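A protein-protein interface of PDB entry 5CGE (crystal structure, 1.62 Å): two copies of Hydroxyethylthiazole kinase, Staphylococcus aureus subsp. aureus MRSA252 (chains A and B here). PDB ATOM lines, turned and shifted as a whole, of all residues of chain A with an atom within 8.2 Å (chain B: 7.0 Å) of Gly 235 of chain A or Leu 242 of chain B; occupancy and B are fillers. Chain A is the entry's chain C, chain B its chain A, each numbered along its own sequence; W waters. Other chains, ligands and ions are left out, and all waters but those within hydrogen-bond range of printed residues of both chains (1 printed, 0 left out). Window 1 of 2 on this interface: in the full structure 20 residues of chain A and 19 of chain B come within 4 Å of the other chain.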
ATOM      1  N   LEU A 181      23.670  32.648 -11.703  1.00  0.00           N
ATOM      2  CA  LEU A 181      22.836  32.289 -12.858  1.00  0.00           C
ATOM      3  C   LEU A 181      23.494  32.516 -14.148  1.00  0.00           C
ATOM      4  O   LEU A 181      23.158  31.922 -15.145  1.00  0.00           O
ATOM      5  CB  LEU A 181      21.517  33.022 -12.817  1.00  0.00           C
ATOM      6  CG  LEU A 181      20.546  32.575 -11.794  1.00  0.00           C
ATOM      7  CD1 LEU A 181      19.300  33.427 -11.767  1.00  0.00           C
ATOM      8  CD2 LEU A 181      20.153  31.109 -11.981  1.00  0.00           C
ATOM      9  N   ARG A 184      24.618  29.484 -16.076  1.00  0.00           N
ATOM     10  CA  ARG A 184      23.568  28.614 -16.533  1.00  0.00           C
ATOM     11  C   ARG A 184      22.900  29.189 -17.757  1.00  0.00           C
ATOM     12  O   ARG A 184      21.870  28.664 -18.261  1.00  0.00           O
ATOM     13  CB  ARG A 184      22.533  28.401 -15.407  1.00  0.00           C
ATOM     14  CG  ARG A 184      23.151  27.782 -14.148  1.00  0.00           C
ATOM     15  CD  ARG A 184      23.603  26.306 -14.480  1.00  0.00           C
ATOM     16  NE  ARG A 184      25.005  26.047 -14.813  1.00  0.00           N
ATOM     17  CZ  ARG A 184      25.467  24.916 -15.366  1.00  0.00           C
ATOM     18  NH1 ARG A 184      24.691  23.846 -15.672  1.00  0.00           N
ATOM     19  N   VAL A 185      23.496  30.245 -18.301  1.00  0.00           N
ATOM     20  CA  VAL A 185      23.004  30.830 -19.564  1.00  0.00           C
ATOM     21  C   VAL A 185      24.123  30.665 -20.575  1.00  0.00           C
ATOM     22  O   VAL A 185      25.229  31.177 -20.406  1.00  0.00           O
ATOM     23  CB  VAL A 185      22.637  32.309 -19.415  1.00  0.00           C
ATOM     24  CG1 VAL A 185      22.204  32.904 -20.759  1.00  0.00           C
ATOM     25  CG2 VAL A 185      21.528  32.475 -18.395  1.00  0.00           C
ATOM     26  N   ASN A 230      10.741  38.773 -10.499  1.00  0.00           N
ATOM     27  CA  ASN A 230      10.314  37.926 -11.619  1.00  0.00           C
ATOM     28  C   ASN A 230      11.434  37.052 -12.207  1.00  0.00           C
ATOM     29  O   ASN A 230      11.192  36.354 -13.180  1.00  0.00           O
ATOM     30  CB  ASN A 230       9.854  38.825 -12.773  1.00  0.00           C
ATOM     31  CG  ASN A 230       8.772  39.806 -12.369  1.00  0.00           C
ATOM     32  OD1 ASN A 230       7.770  39.403 -11.826  1.00  0.00           O
ATOM     33  ND2 ASN A 230       9.102  41.123 -12.450  1.00  0.00           N
ATOM     34  N   CYS A 231      12.591  37.030 -11.533  1.00  0.00           N
ATOM     35  CA  CYS A 231      13.577  36.052 -11.914  1.00  0.00           C
ATOM     36  C   CYS A 231      13.399  34.740 -11.234  1.00  0.00           C
ATOM     37  O   CYS A 231      13.607  34.636  -9.985  1.00  0.00           O
ATOM     38  CB  CYS A 231      14.944  36.584 -11.584  1.00  0.00           C
ATOM     39  SG  CYS A 231      16.311  35.553 -12.190  1.00  0.00           S
ATOM     40  N   GLY A 232      13.018  33.743 -12.013  1.00  0.00           N
ATOM     41  CA  GLY A 232      12.686  32.425 -11.454  1.00  0.00           C
ATOM     42  C   GLY A 232      13.676  31.343 -11.802  1.00  0.00           C
ATOM     43  O   GLY A 232      13.480  30.178 -11.405  1.00  0.00           O
ATOM     44  N   GLY A 233      14.759  31.713 -12.482  1.00  0.00           N
ATOM     45  CA  GLY A 233      15.730  30.738 -12.866  1.00  0.00           C
ATOM     46  C   GLY A 233      16.483  31.199 -14.081  1.00  0.00           C
ATOM     47  O   GLY A 233      16.308  32.342 -14.464  1.00  0.00           O
ATOM     48  N   PRO A 234      17.289  30.361 -14.631  1.00  0.00           N
ATOM     49  CA  PRO A 234      18.129  30.769 -15.749  1.00  0.00           C
ATOM     50  C   PRO A 234      17.338  31.170 -16.988  1.00  0.00           C
ATOM     51  O   PRO A 234      17.817  31.973 -17.789  1.00  0.00           O
ATOM     52  CB  PRO A 234      18.991  29.554 -16.061  1.00  0.00           C
ATOM     53  CG  PRO A 234      18.348  28.460 -15.403  1.00  0.00           C
ATOM     54  CD  PRO A 234      17.484  28.938 -14.284  1.00  0.00           C
ATOM     55  N   GLY A 235      16.127  30.630 -17.169  1.00  0.00           N
ATOM     56  CA  GLY A 235      15.317  30.991 -18.324  1.00  0.00           C
ATOM     57  C   GLY A 235      14.832  32.396 -18.238  1.00  0.00           C
ATOM     58  O   GLY A 235      14.920  33.163 -19.197  1.00  0.00           O
ATOM     59  N   THR A 236      14.227  32.780 -17.139  1.00  0.00           N
ATOM     60  CA  THR A 236      13.651  34.122 -17.021  1.00  0.00           C
ATOM     61  C   THR A 236      14.768  35.134 -16.807  1.00  0.00           C
ATOM     62  O   THR A 236      14.588  36.293 -17.074  1.00  0.00           O
ATOM     63  CB  THR A 236      12.534  34.175 -15.969  1.00  0.00           C
ATOM     64  OG1 THR A 236      12.985  33.507 -14.794  1.00  0.00           O
ATOM     65  CG2 THR A 236      11.295  33.556 -16.500  1.00  0.00           C
ATOM     66  N   PHE A 237      15.891  34.658 -16.310  1.00  0.00           N
ATOM     67  CA  PHE A 237      17.018  35.588 -16.049  1.00  0.00           C
ATOM     68  C   PHE A 237      17.525  36.214 -17.300  1.00  0.00           C
ATOM     69  O   PHE A 237      17.854  37.401 -17.291  1.00  0.00           O
ATOM     70  CB  PHE A 237      18.145  34.792 -15.376  1.00  0.00           C
ATOM     71  CG  PHE A 237      19.447  35.522 -15.309  1.00  0.00           C
ATOM     72  CD1 PHE A 237      19.693  36.415 -14.280  1.00  0.00           C
ATOM     73  CD2 PHE A 237      20.467  35.170 -16.117  1.00  0.00           C
ATOM     74  CE1 PHE A 237      20.904  37.062 -14.174  1.00  0.00           C
ATOM     75  CE2 PHE A 237      21.703  35.838 -16.041  1.00  0.00           C
ATOM     76  CZ  PHE A 237      21.879  36.799 -15.064  1.00  0.00           C
ATOM     77  N   SER A 238      17.569  35.471 -18.372  1.00  0.00           N
ATOM     78  CA  SER A 238      18.167  36.018 -19.605  1.00  0.00           C
ATOM     79  C   SER A 238      17.415  37.264 -20.155  1.00  0.00           C
ATOM     80  O   SER A 238      18.009  38.320 -20.378  1.00  0.00           O
ATOM     81  CB  SER A 238      18.315  34.893 -20.598  1.00  0.00           C
ATOM     82  OG  SER A 238      18.813  35.417 -21.803  1.00  0.00           O
ATOM     83  N   PRO A 239      16.048  37.220 -20.344  1.00  0.00           N
ATOM     84  CA  PRO A 239      15.345  38.415 -20.682  1.00  0.00           C
ATOM     85  C   PRO A 239      15.604  39.551 -19.682  1.00  0.00           C
ATOM     86  O   PRO A 239      15.705  40.745 -20.057  1.00  0.00           O
ATOM     87  CB  PRO A 239      13.887  37.972 -20.687  1.00  0.00           C
ATOM     88  CG  PRO A 239      13.995  36.554 -21.037  1.00  0.00           C
ATOM     89  CD  PRO A 239      15.202  36.013 -20.385  1.00  0.00           C
ATOM     90  N   LEU A 240      15.619  39.268 -18.384  1.00  0.00           N
ATOM     91  CA  LEU A 240      15.775  40.275 -17.379  1.00  0.00           C
ATOM     92  C   LEU A 240      17.167  40.897 -17.445  1.00  0.00           C
ATOM     93  O   LEU A 240      17.298  42.039 -17.123  1.00  0.00           O
ATOM     94  CB  LEU A 240      15.477  39.706 -15.999  1.00  0.00           C
ATOM     95  CG  LEU A 240      14.030  39.331 -15.790  1.00  0.00           C
ATOM     96  CD1 LEU A 240      13.855  38.573 -14.484  1.00  0.00           C
ATOM     97  CD2 LEU A 240      13.102  40.525 -15.774  1.00  0.00           C
ATOM     98  N   LEU A 241      18.151  40.094 -17.776  1.00  0.00           N
ATOM     99  CA  LEU A 241      19.544  40.646 -17.953  1.00  0.00           C
ATOM    100  C   LEU A 241      19.509  41.711 -19.001  1.00  0.00           C
ATOM    101  O   LEU A 241      20.118  42.779 -18.834  1.00  0.00           O
ATOM    102  CB  LEU A 241      20.516  39.494 -18.219  1.00  0.00           C
ATOM    103  CG  LEU A 241      21.925  39.922 -18.642  1.00  0.00           C
ATOM    104  CD1 LEU A 241      22.607  40.622 -17.463  1.00  0.00           C
ATOM    105  CD2 LEU A 241      22.744  38.705 -19.092  1.00  0.00           C
ATOM    106  N   ASN B  24      21.081  27.289 -29.589  1.00  0.00           N
ATOM    107  CA  ASN B  24      21.073  28.056 -28.333  1.00  0.00           C
ATOM    108  C   ASN B  24      20.074  27.415 -27.352  1.00  0.00           C
ATOM    109  O   ASN B  24      20.347  27.275 -26.187  1.00  0.00           O
ATOM    110  CB  ASN B  24      20.696  29.490 -28.643  1.00  0.00           C
ATOM    111  CG  ASN B  24      20.553  30.307 -27.388  1.00  0.00           C
ATOM    112  OD1 ASN B  24      19.446  30.395 -26.804  1.00  0.00           O
ATOM    113  ND2 ASN B  24      21.644  30.878 -26.917  1.00  0.00           N
ATOM    114  N   PHE B  25      18.869  27.110 -27.835  1.00  0.00           N
ATOM    115  CA  PHE B  25      17.881  26.549 -26.911  1.00  0.00           C
ATOM    116  C   PHE B  25      18.314  25.194 -26.398  1.00  0.00           C
ATOM    117  O   PHE B  25      18.067  24.849 -25.222  1.00  0.00           O
ATOM    118  CB  PHE B  25      16.545  26.423 -27.690  1.00  0.00           C
ATOM    119  CG  PHE B  25      15.358  26.081 -26.850  1.00  0.00           C
ATOM    120  CD1 PHE B  25      15.062  26.794 -25.694  1.00  0.00           C
ATOM    121  CD2 PHE B  25      14.613  25.034 -27.205  1.00  0.00           C
ATOM    122  CE1 PHE B  25      13.999  26.512 -24.911  1.00  0.00           C
ATOM    123  CE2 PHE B  25      13.435  24.783 -26.471  1.00  0.00           C
ATOM    124  CZ  PHE B  25      13.223  25.474 -25.276  1.00  0.00           C
ATOM    125  N   THR B  26      18.900  24.384 -27.239  1.00  0.00           N
ATOM    126  CA  THR B  26      19.386  23.071 -26.828  1.00  0.00           C
ATOM    127  C   THR B  26      20.455  23.233 -25.724  1.00  0.00           C
ATOM    128  O   THR B  26      20.441  22.560 -24.710  1.00  0.00           O
ATOM    129  CB  THR B  26      19.956  22.291 -28.008  1.00  0.00           C
ATOM    130  OG1 THR B  26      18.900  22.090 -28.964  1.00  0.00           O
ATOM    131  CG2 THR B  26      20.439  20.972 -27.588  1.00  0.00           C
ATOM    132  N   ALA B  27      21.394  24.119 -25.973  1.00  0.00           N
ATOM    133  CA  ALA B  27      22.425  24.352 -24.945  1.00  0.00           C
ATOM    134  C   ALA B  27      21.845  24.858 -23.653  1.00  0.00           C
ATOM    135  O   ALA B  27      22.234  24.423 -22.570  1.00  0.00           O
ATOM    136  CB  ALA B  27      23.489  25.324 -25.485  1.00  0.00           C
ATOM    137  N   ASN B  28      20.886  25.797 -23.727  1.00  0.00           N
ATOM    138  CA  ASN B  28      20.279  26.299 -22.511  1.00  0.00           C
ATOM    139  C   ASN B  28      19.468  25.253 -21.764  1.00  0.00           C
ATOM    140  O   ASN B  28      19.474  25.247 -20.582  1.00  0.00           O
ATOM    141  CB  ASN B  28      19.444  27.529 -22.804  1.00  0.00           C
ATOM    142  CG  ASN B  28      20.351  28.782 -22.935  1.00  0.00           C
ATOM    143  OD1 ASN B  28      21.298  28.895 -22.161  1.00  0.00           O
ATOM    144  ND2 ASN B  28      20.120  29.660 -23.846  1.00  0.00           N
ATOM    145  N   GLY B  29      18.818  24.415 -22.530  1.00  0.00           N
ATOM    146  CA  GLY B  29      18.095  23.348 -21.848  1.00  0.00           C
ATOM    147  C   GLY B  29      18.989  22.352 -21.168  1.00  0.00           C
ATOM    148  O   GLY B  29      18.730  21.947 -20.047  1.00  0.00           O
ATOM    149  N   LEU B  30      20.096  22.000 -21.803  1.00  0.00           N
ATOM    150  CA  LEU B  30      21.062  21.145 -21.167  1.00  0.00           C
ATOM    151  C   LEU B  30      21.682  21.810 -19.973  1.00  0.00           C
ATOM    152  O   LEU B  30      21.835  21.217 -18.930  1.00  0.00           O
ATOM    153  CB  LEU B  30      22.131  20.751 -22.192  1.00  0.00           C
ATOM    154  CG  LEU B  30      21.696  19.564 -23.059  1.00  0.00           C
ATOM    155  CD1 LEU B  30      22.599  19.450 -24.296  1.00  0.00           C
ATOM    156  CD2 LEU B  30      21.636  18.261 -22.250  1.00  0.00           C
ATOM    157  N   SER B  32      20.208  23.967 -18.059  1.00  0.00           N
ATOM    158  CA  SER B  32      19.182  24.049 -17.035  1.00  0.00           C
ATOM    159  C   SER B  32      19.101  22.765 -16.213  1.00  0.00           C
ATOM    160  O   SER B  32      18.822  22.885 -14.989  1.00  0.00           O
ATOM    161  CB  SER B  32      17.839  24.466 -17.629  1.00  0.00           C
ATOM    162  OG  SER B  32      17.202  23.346 -18.275  1.00  0.00           O
ATOM    163  N   ILE B  33      19.332  21.603 -16.799  1.00  0.00           N
ATOM    164  CA  ILE B  33      19.294  20.372 -16.027  1.00  0.00           C
ATOM    165  C   ILE B  33      20.647  20.011 -15.434  1.00  0.00           C
ATOM    166  O   ILE B  33      20.776  18.975 -14.811  1.00  0.00           O
ATOM    167  CB  ILE B  33      18.788  19.176 -16.798  1.00  0.00           C
ATOM    168  CG1 ILE B  33      19.657  18.833 -18.049  1.00  0.00           C
ATOM    169  CG2 ILE B  33      17.339  19.424 -17.231  1.00  0.00           C
ATOM    170  CD1 ILE B  33      19.283  17.506 -18.709  1.00  0.00           C
ATOM    171  N   LEU B 191      15.485  19.934 -28.498  1.00  0.00           N
ATOM    172  CA  LEU B 191      15.962  20.004 -27.173  1.00  0.00           C
ATOM    173  C   LEU B 191      15.734  18.654 -26.435  1.00  0.00           C
ATOM    174  O   LEU B 191      16.652  18.149 -25.761  1.00  0.00           O
ATOM    175  CB  LEU B 191      15.355  21.118 -26.362  1.00  0.00           C
ATOM    176  CG  LEU B 191      15.576  21.082 -24.849  1.00  0.00           C
ATOM    177  CD1 LEU B 191      17.098  21.004 -24.488  1.00  0.00           C
ATOM    178  CD2 LEU B 191      14.921  22.288 -24.174  1.00  0.00           C
ATOM    179  N   ALA B 221       8.173  19.086 -16.815  1.00  0.00           N
ATOM    180  CA  ALA B 221       8.538  20.496 -16.751  1.00  0.00           C
ATOM    181  C   ALA B 221       7.650  21.366 -17.632  1.00  0.00           C
ATOM    182  O   ALA B 221       7.303  22.457 -17.279  1.00  0.00           O
ATOM    183  CB  ALA B 221      10.024  20.692 -17.101  1.00  0.00           C
ATOM    184  N   ALA B 225       5.388  24.359 -16.338  1.00  0.00           N
ATOM    185  CA  ALA B 225       5.633  25.702 -16.823  1.00  0.00           C
ATOM    186  C   ALA B 225       4.389  26.329 -17.421  1.00  0.00           C
ATOM    187  O   ALA B 225       4.153  27.499 -17.225  1.00  0.00           O
ATOM    188  CB  ALA B 225       6.702  25.644 -17.891  1.00  0.00           C
ATOM    189  N   PHE B 237       6.397  31.047 -22.349  1.00  0.00           N
ATOM    190  CA  PHE B 237       6.578  29.686 -21.967  1.00  0.00           C
ATOM    191  C   PHE B 237       8.000  29.167 -22.005  1.00  0.00           C
ATOM    192  O   PHE B 237       8.440  28.423 -21.139  1.00  0.00           O
ATOM    193  CB  PHE B 237       5.676  28.802 -22.866  1.00  0.00           C
ATOM    194  CG  PHE B 237       5.907  27.322 -22.759  1.00  0.00           C
ATOM    195  CD1 PHE B 237       5.302  26.611 -21.710  1.00  0.00           C
ATOM    196  CD2 PHE B 237       6.636  26.647 -23.657  1.00  0.00           C
ATOM    197  CE1 PHE B 237       5.533  25.230 -21.552  1.00  0.00           C
ATOM    198  CE2 PHE B 237       6.743  25.267 -23.583  1.00  0.00           C
ATOM    199  CZ  PHE B 237       6.210  24.564 -22.523  1.00  0.00           C
ATOM    200  N   SER B 238       8.730  29.586 -23.038  1.00  0.00           N
ATOM    201  CA  SER B 238      10.059  29.037 -23.212  1.00  0.00           C
ATOM    202  C   SER B 238      11.011  29.381 -22.012  1.00  0.00           C
ATOM    203  O   SER B 238      11.654  28.456 -21.457  1.00  0.00           O
ATOM    204  CB  SER B 238      10.567  29.495 -24.534  1.00  0.00           C
ATOM    205  OG  SER B 238      11.912  29.075 -24.684  1.00  0.00           O
ATOM    206  N   PRO B 239      11.137  30.639 -21.614  1.00  0.00           N
ATOM    207  CA  PRO B 239      11.879  30.941 -20.360  1.00  0.00           C
ATOM    208  C   PRO B 239      11.404  30.168 -19.151  1.00  0.00           C
ATOM    209  O   PRO B 239      12.193  29.695 -18.335  1.00  0.00           O
ATOM    210  CB  PRO B 239      11.669  32.484 -20.151  1.00  0.00           C
ATOM    211  CG  PRO B 239      11.502  32.944 -21.532  1.00  0.00           C
ATOM    212  CD  PRO B 239      10.710  31.879 -22.271  1.00  0.00           C
ATOM    213  N   LEU B 240      10.078  30.008 -19.027  1.00  0.00           N
ATOM    214  CA  LEU B 240       9.568  29.324 -17.897  1.00  0.00           C
ATOM    215  C   LEU B 240       9.851  27.808 -17.958  1.00  0.00           C
ATOM    216  O   LEU B 240      10.013  27.211 -16.928  1.00  0.00           O
ATOM    217  CB  LEU B 240       8.037  29.562 -17.791  1.00  0.00           C
ATOM    218  CG  LEU B 240       7.665  30.991 -17.462  1.00  0.00           C
ATOM    219  CD1 LEU B 240       6.154  31.215 -17.623  1.00  0.00           C
ATOM    220  CD2 LEU B 240       8.067  31.432 -16.074  1.00  0.00           C
ATOM    221  N   LEU B 241       9.873  27.228 -19.125  1.00  0.00           N
ATOM    222  CA  LEU B 241      10.253  25.863 -19.260  1.00  0.00           C
ATOM    223  C   LEU B 241      11.675  25.660 -18.708  1.00  0.00           C
ATOM    224  O   LEU B 241      11.966  24.659 -18.008  1.00  0.00           O
ATOM    225  CB  LEU B 241      10.131  25.398 -20.695  1.00  0.00           C
ATOM    226  CG  LEU B 241      10.688  24.080 -21.083  1.00  0.00           C
ATOM    227  CD1 LEU B 241       9.917  22.968 -20.375  1.00  0.00           C
ATOM    228  CD2 LEU B 241      10.671  23.808 -22.575  1.00  0.00           C
ATOM    229  N   LEU B 242      12.561  26.526 -19.126  1.00  0.00           N
ATOM    230  CA  LEU B 242      13.958  26.408 -18.670  1.00  0.00           C
ATOM    231  C   LEU B 242      14.033  26.579 -17.146  1.00  0.00           C
ATOM    232  O   LEU B 242      14.787  25.817 -16.476  1.00  0.00           O
ATOM    233  CB  LEU B 242      14.849  27.436 -19.360  1.00  0.00           C
ATOM    234  CG  LEU B 242      15.021  27.271 -20.839  1.00  0.00           C
ATOM    235  CD1 LEU B 242      15.719  28.433 -21.515  1.00  0.00           C
ATOM    236  CD2 LEU B 242      15.664  25.950 -21.182  1.00  0.00           C
ATOM    237  N   ASP B 243      13.288  27.496 -16.578  1.00  0.00           N
ATOM    238  CA  ASP B 243      13.253  27.663 -15.123  1.00  0.00           C
ATOM    239  C   ASP B 243      12.723  26.394 -14.448  1.00  0.00           C
ATOM    240  O   ASP B 243      13.227  25.974 -13.417  1.00  0.00           O
ATOM    241  CB  ASP B 243      12.337  28.749 -14.668  1.00  0.00           C
ATOM    242  CG  ASP B 243      12.842  30.170 -14.920  1.00  0.00           C
ATOM    243  OD1 ASP B 243      13.971  30.347 -15.456  1.00  0.00           O
ATOM    244  OD2 ASP B 243      12.023  31.108 -14.597  1.00  0.00           O
ATOM    245  N   THR B 244      11.666  25.794 -15.062  1.00  0.00           N
ATOM    246  CA  THR B 244      11.056  24.633 -14.425  1.00  0.00           C
ATOM    247  C   THR B 244      11.938  23.400 -14.512  1.00  0.00           C
ATOM    248  O   THR B 244      12.039  22.666 -13.530  1.00  0.00           O
ATOM    249  CB  THR B 244       9.682  24.363 -15.097  1.00  0.00           C
ATOM    250  OG1 THR B 244       8.886  25.579 -15.017  1.00  0.00           O
ATOM    251  CG2 THR B 244       8.992  23.256 -14.394  1.00  0.00           C
ATOM    252  N   LEU B 245      12.720  23.243 -15.585  1.00  0.00           N
ATOM    253  CA  LEU B 245      13.719  22.191 -15.652  1.00  0.00           C
ATOM    254  C   LEU B 245      14.787  22.432 -14.554  1.00  0.00           C
ATOM    255  O   LEU B 245      15.221  21.499 -13.920  1.00  0.00           O
ATOM    256  CB  LEU B 245      14.412  22.212 -17.027  1.00  0.00           C
ATOM    257  CG  LEU B 245      13.580  21.657 -18.171  1.00  0.00           C
ATOM    258  CD1 LEU B 245      14.213  22.033 -19.494  1.00  0.00           C
ATOM    259  CD2 LEU B 245      13.493  20.152 -18.042  1.00  0.00           C
ATOM    260  N   TYR B 246      15.139  23.663 -14.353  1.00  0.00           N
ATOM    261  CA  TYR B 246      16.250  23.974 -13.407  1.00  0.00           C
ATOM    262  C   TYR B 246      15.843  23.596 -12.001  1.00  0.00           C
ATOM    263  O   TYR B 246      16.688  23.123 -11.231  1.00  0.00           O
ATOM    264  CB  TYR B 246      16.605  25.437 -13.520  1.00  0.00           C
ATOM    265  CG  TYR B 246      17.671  25.934 -12.589  1.00  0.00           C
ATOM    266  CD1 TYR B 246      18.968  25.582 -12.814  1.00  0.00           C
ATOM    267  CD2 TYR B 246      17.349  26.730 -11.531  1.00  0.00           C
ATOM    268  CE1 TYR B 246      19.964  26.129 -12.027  1.00  0.00           C
ATOM    269  CE2 TYR B 246      18.352  27.296 -10.744  1.00  0.00           C
ATOM    270  CZ  TYR B 246      19.590  26.900 -10.954  1.00  0.00           C
ATOM    271  OH  TYR B 246      20.626  27.453 -10.156  1.00  0.00           O
ATOM    272  N   HIS B 247      14.579  23.829 -11.666  1.00  0.00           N
ATOM    273  CA  HIS B 247      14.018  23.661 -10.293  1.00  0.00           C
ATOM    274  C   HIS B 247      13.284  22.333 -10.095  1.00  0.00           C
ATOM    275  O   HIS B 247      12.968  22.016  -8.937  1.00  0.00           O
ATOM    276  CB  HIS B 247      13.110  24.770  -9.935  1.00  0.00           C
ATOM    277  CG  HIS B 247      13.792  26.070  -9.711  1.00  0.00           C
ATOM    278  ND1 HIS B 247      14.674  26.271  -8.672  1.00  0.00           N
ATOM    279  CD2 HIS B 247      13.677  27.261 -10.353  1.00  0.00           C
ATOM    280  CE1 HIS B 247      15.164  27.512  -8.748  1.00  0.00           C
ATOM    281  NE2 HIS B 247      14.550  28.124  -9.778  1.00  0.00           N
HETATM  282  O   HOH W   1      19.513  27.764 -19.124  1.00  0.00           O
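N of Gly 233 of chain A lies close to OD1 of Asp 243 of chain B (3.4 Å). The side-chain carboxylate (OD1) of Asp 243 of chain B lies within hydrogen-bond range of the backbone NH (N) of Gly 235 of chain A (2.8 Å). OD2 of Asp 243 of chain B sits at hydrogen-bond distance from OG1 of Thr 236 of chain A, 2.6 Å away. A ring nitrogen (NE2) of His 247 of chain B is in hydrogen-bond range of the backbone carbonyl oxygen of Gly 232 of chain A (2.8 Å). The backbone nitrogen of Pro 234 of chain A lies close to the side-chain carboxylate of Asp 243 of chain B, 3.4 Å away.
The side-chain amide oxygen of Asn 24 of chain B sits at hydrogen-bond distance from the side-chain amide nitrogen of Asn 28 of chain B, at 3.1 Å. O of Leu 240 of chain B sits at hydrogen-bond distance from OG1 of Thr 244 of chain B (2.8 Å). The backbone NH (N) of Gly 232 of chain A sits at hydrogen-bond distance from the side-chain hydroxyl (OG1) of Thr 236 of chain A, 2.8 Å away. N of Gly 233 of chain A sits at hydrogen-bond distance from OG1 of Thr 236 of chain A, 3.4 Å away.
Among the printed residues, merely in contact across the chains: Arg 184 of chain A with Asn 28 of chain B, Val 185 of chain A with Asn 28 of chain B, Gly 232 of chain A with Asp 243 of chain B, Pro 234 of chain A with Tyr 246 of chain B, Gly 235 of chain A with Pro 239 of chain B, Gly 235 of chain A with Leu 242 of chain B, Thr 236 of chain A with Pro 239 of chain B and Thr 236 of chain A with Leu 240 of chain B.
Of chain B, only Pro 239, Leu 242 and Asp 243 come within 4 Å of Gly 235 of chain A. Leu 242 of chain B touches one residue of chain A. Printed residues of chain B within 4 Å of Arg 184 of chain A: Asn 28. Printed residues of chain B within 4 Å of Thr 236 of chain A: Pro 239, Leu 240 and Asp 243. Of the printed residues of chain A, Asp 243 of chain B touches Gly 232, Gly 233, Pro 234, Gly 235 and Thr 236. Of the printed residues of chain A, Tyr 246 of chain B touches Pro 234 (3.5 Å). Leu 241 of chain B touches none of the printed residues of chain A. The nearest residue of chain B that does not touch Gly 235 of chain A is Leu 240 of chain B (5.4 Å). The nearest residue of chain A that does not touch Leu 242 of chain B is Pro 234 of chain A (4.6 Å). The nearest printed residue of chain B that does not touch Val 185 of chain A is Asn 24 of chain B (6.5 Å).
Hydrophobic or aromatic side chains of chain A that line the printed part of chain B: Pro 234. Along chain A the printed residues that touch a printed residue of chain B span positions 184 to 236. Along chain B the printed residues that touch a printed residue of chain A span positions 28 to 247.
5 positions are printed for both chains. Of the 13 pairs that touch across the chains among the printed residues, none has its exchanged pair printed and touching as well.
Water W1 bridges O of Arg 184 of chain A (2.7 Å) and O of Asn 28 of chain B (2.9 Å).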
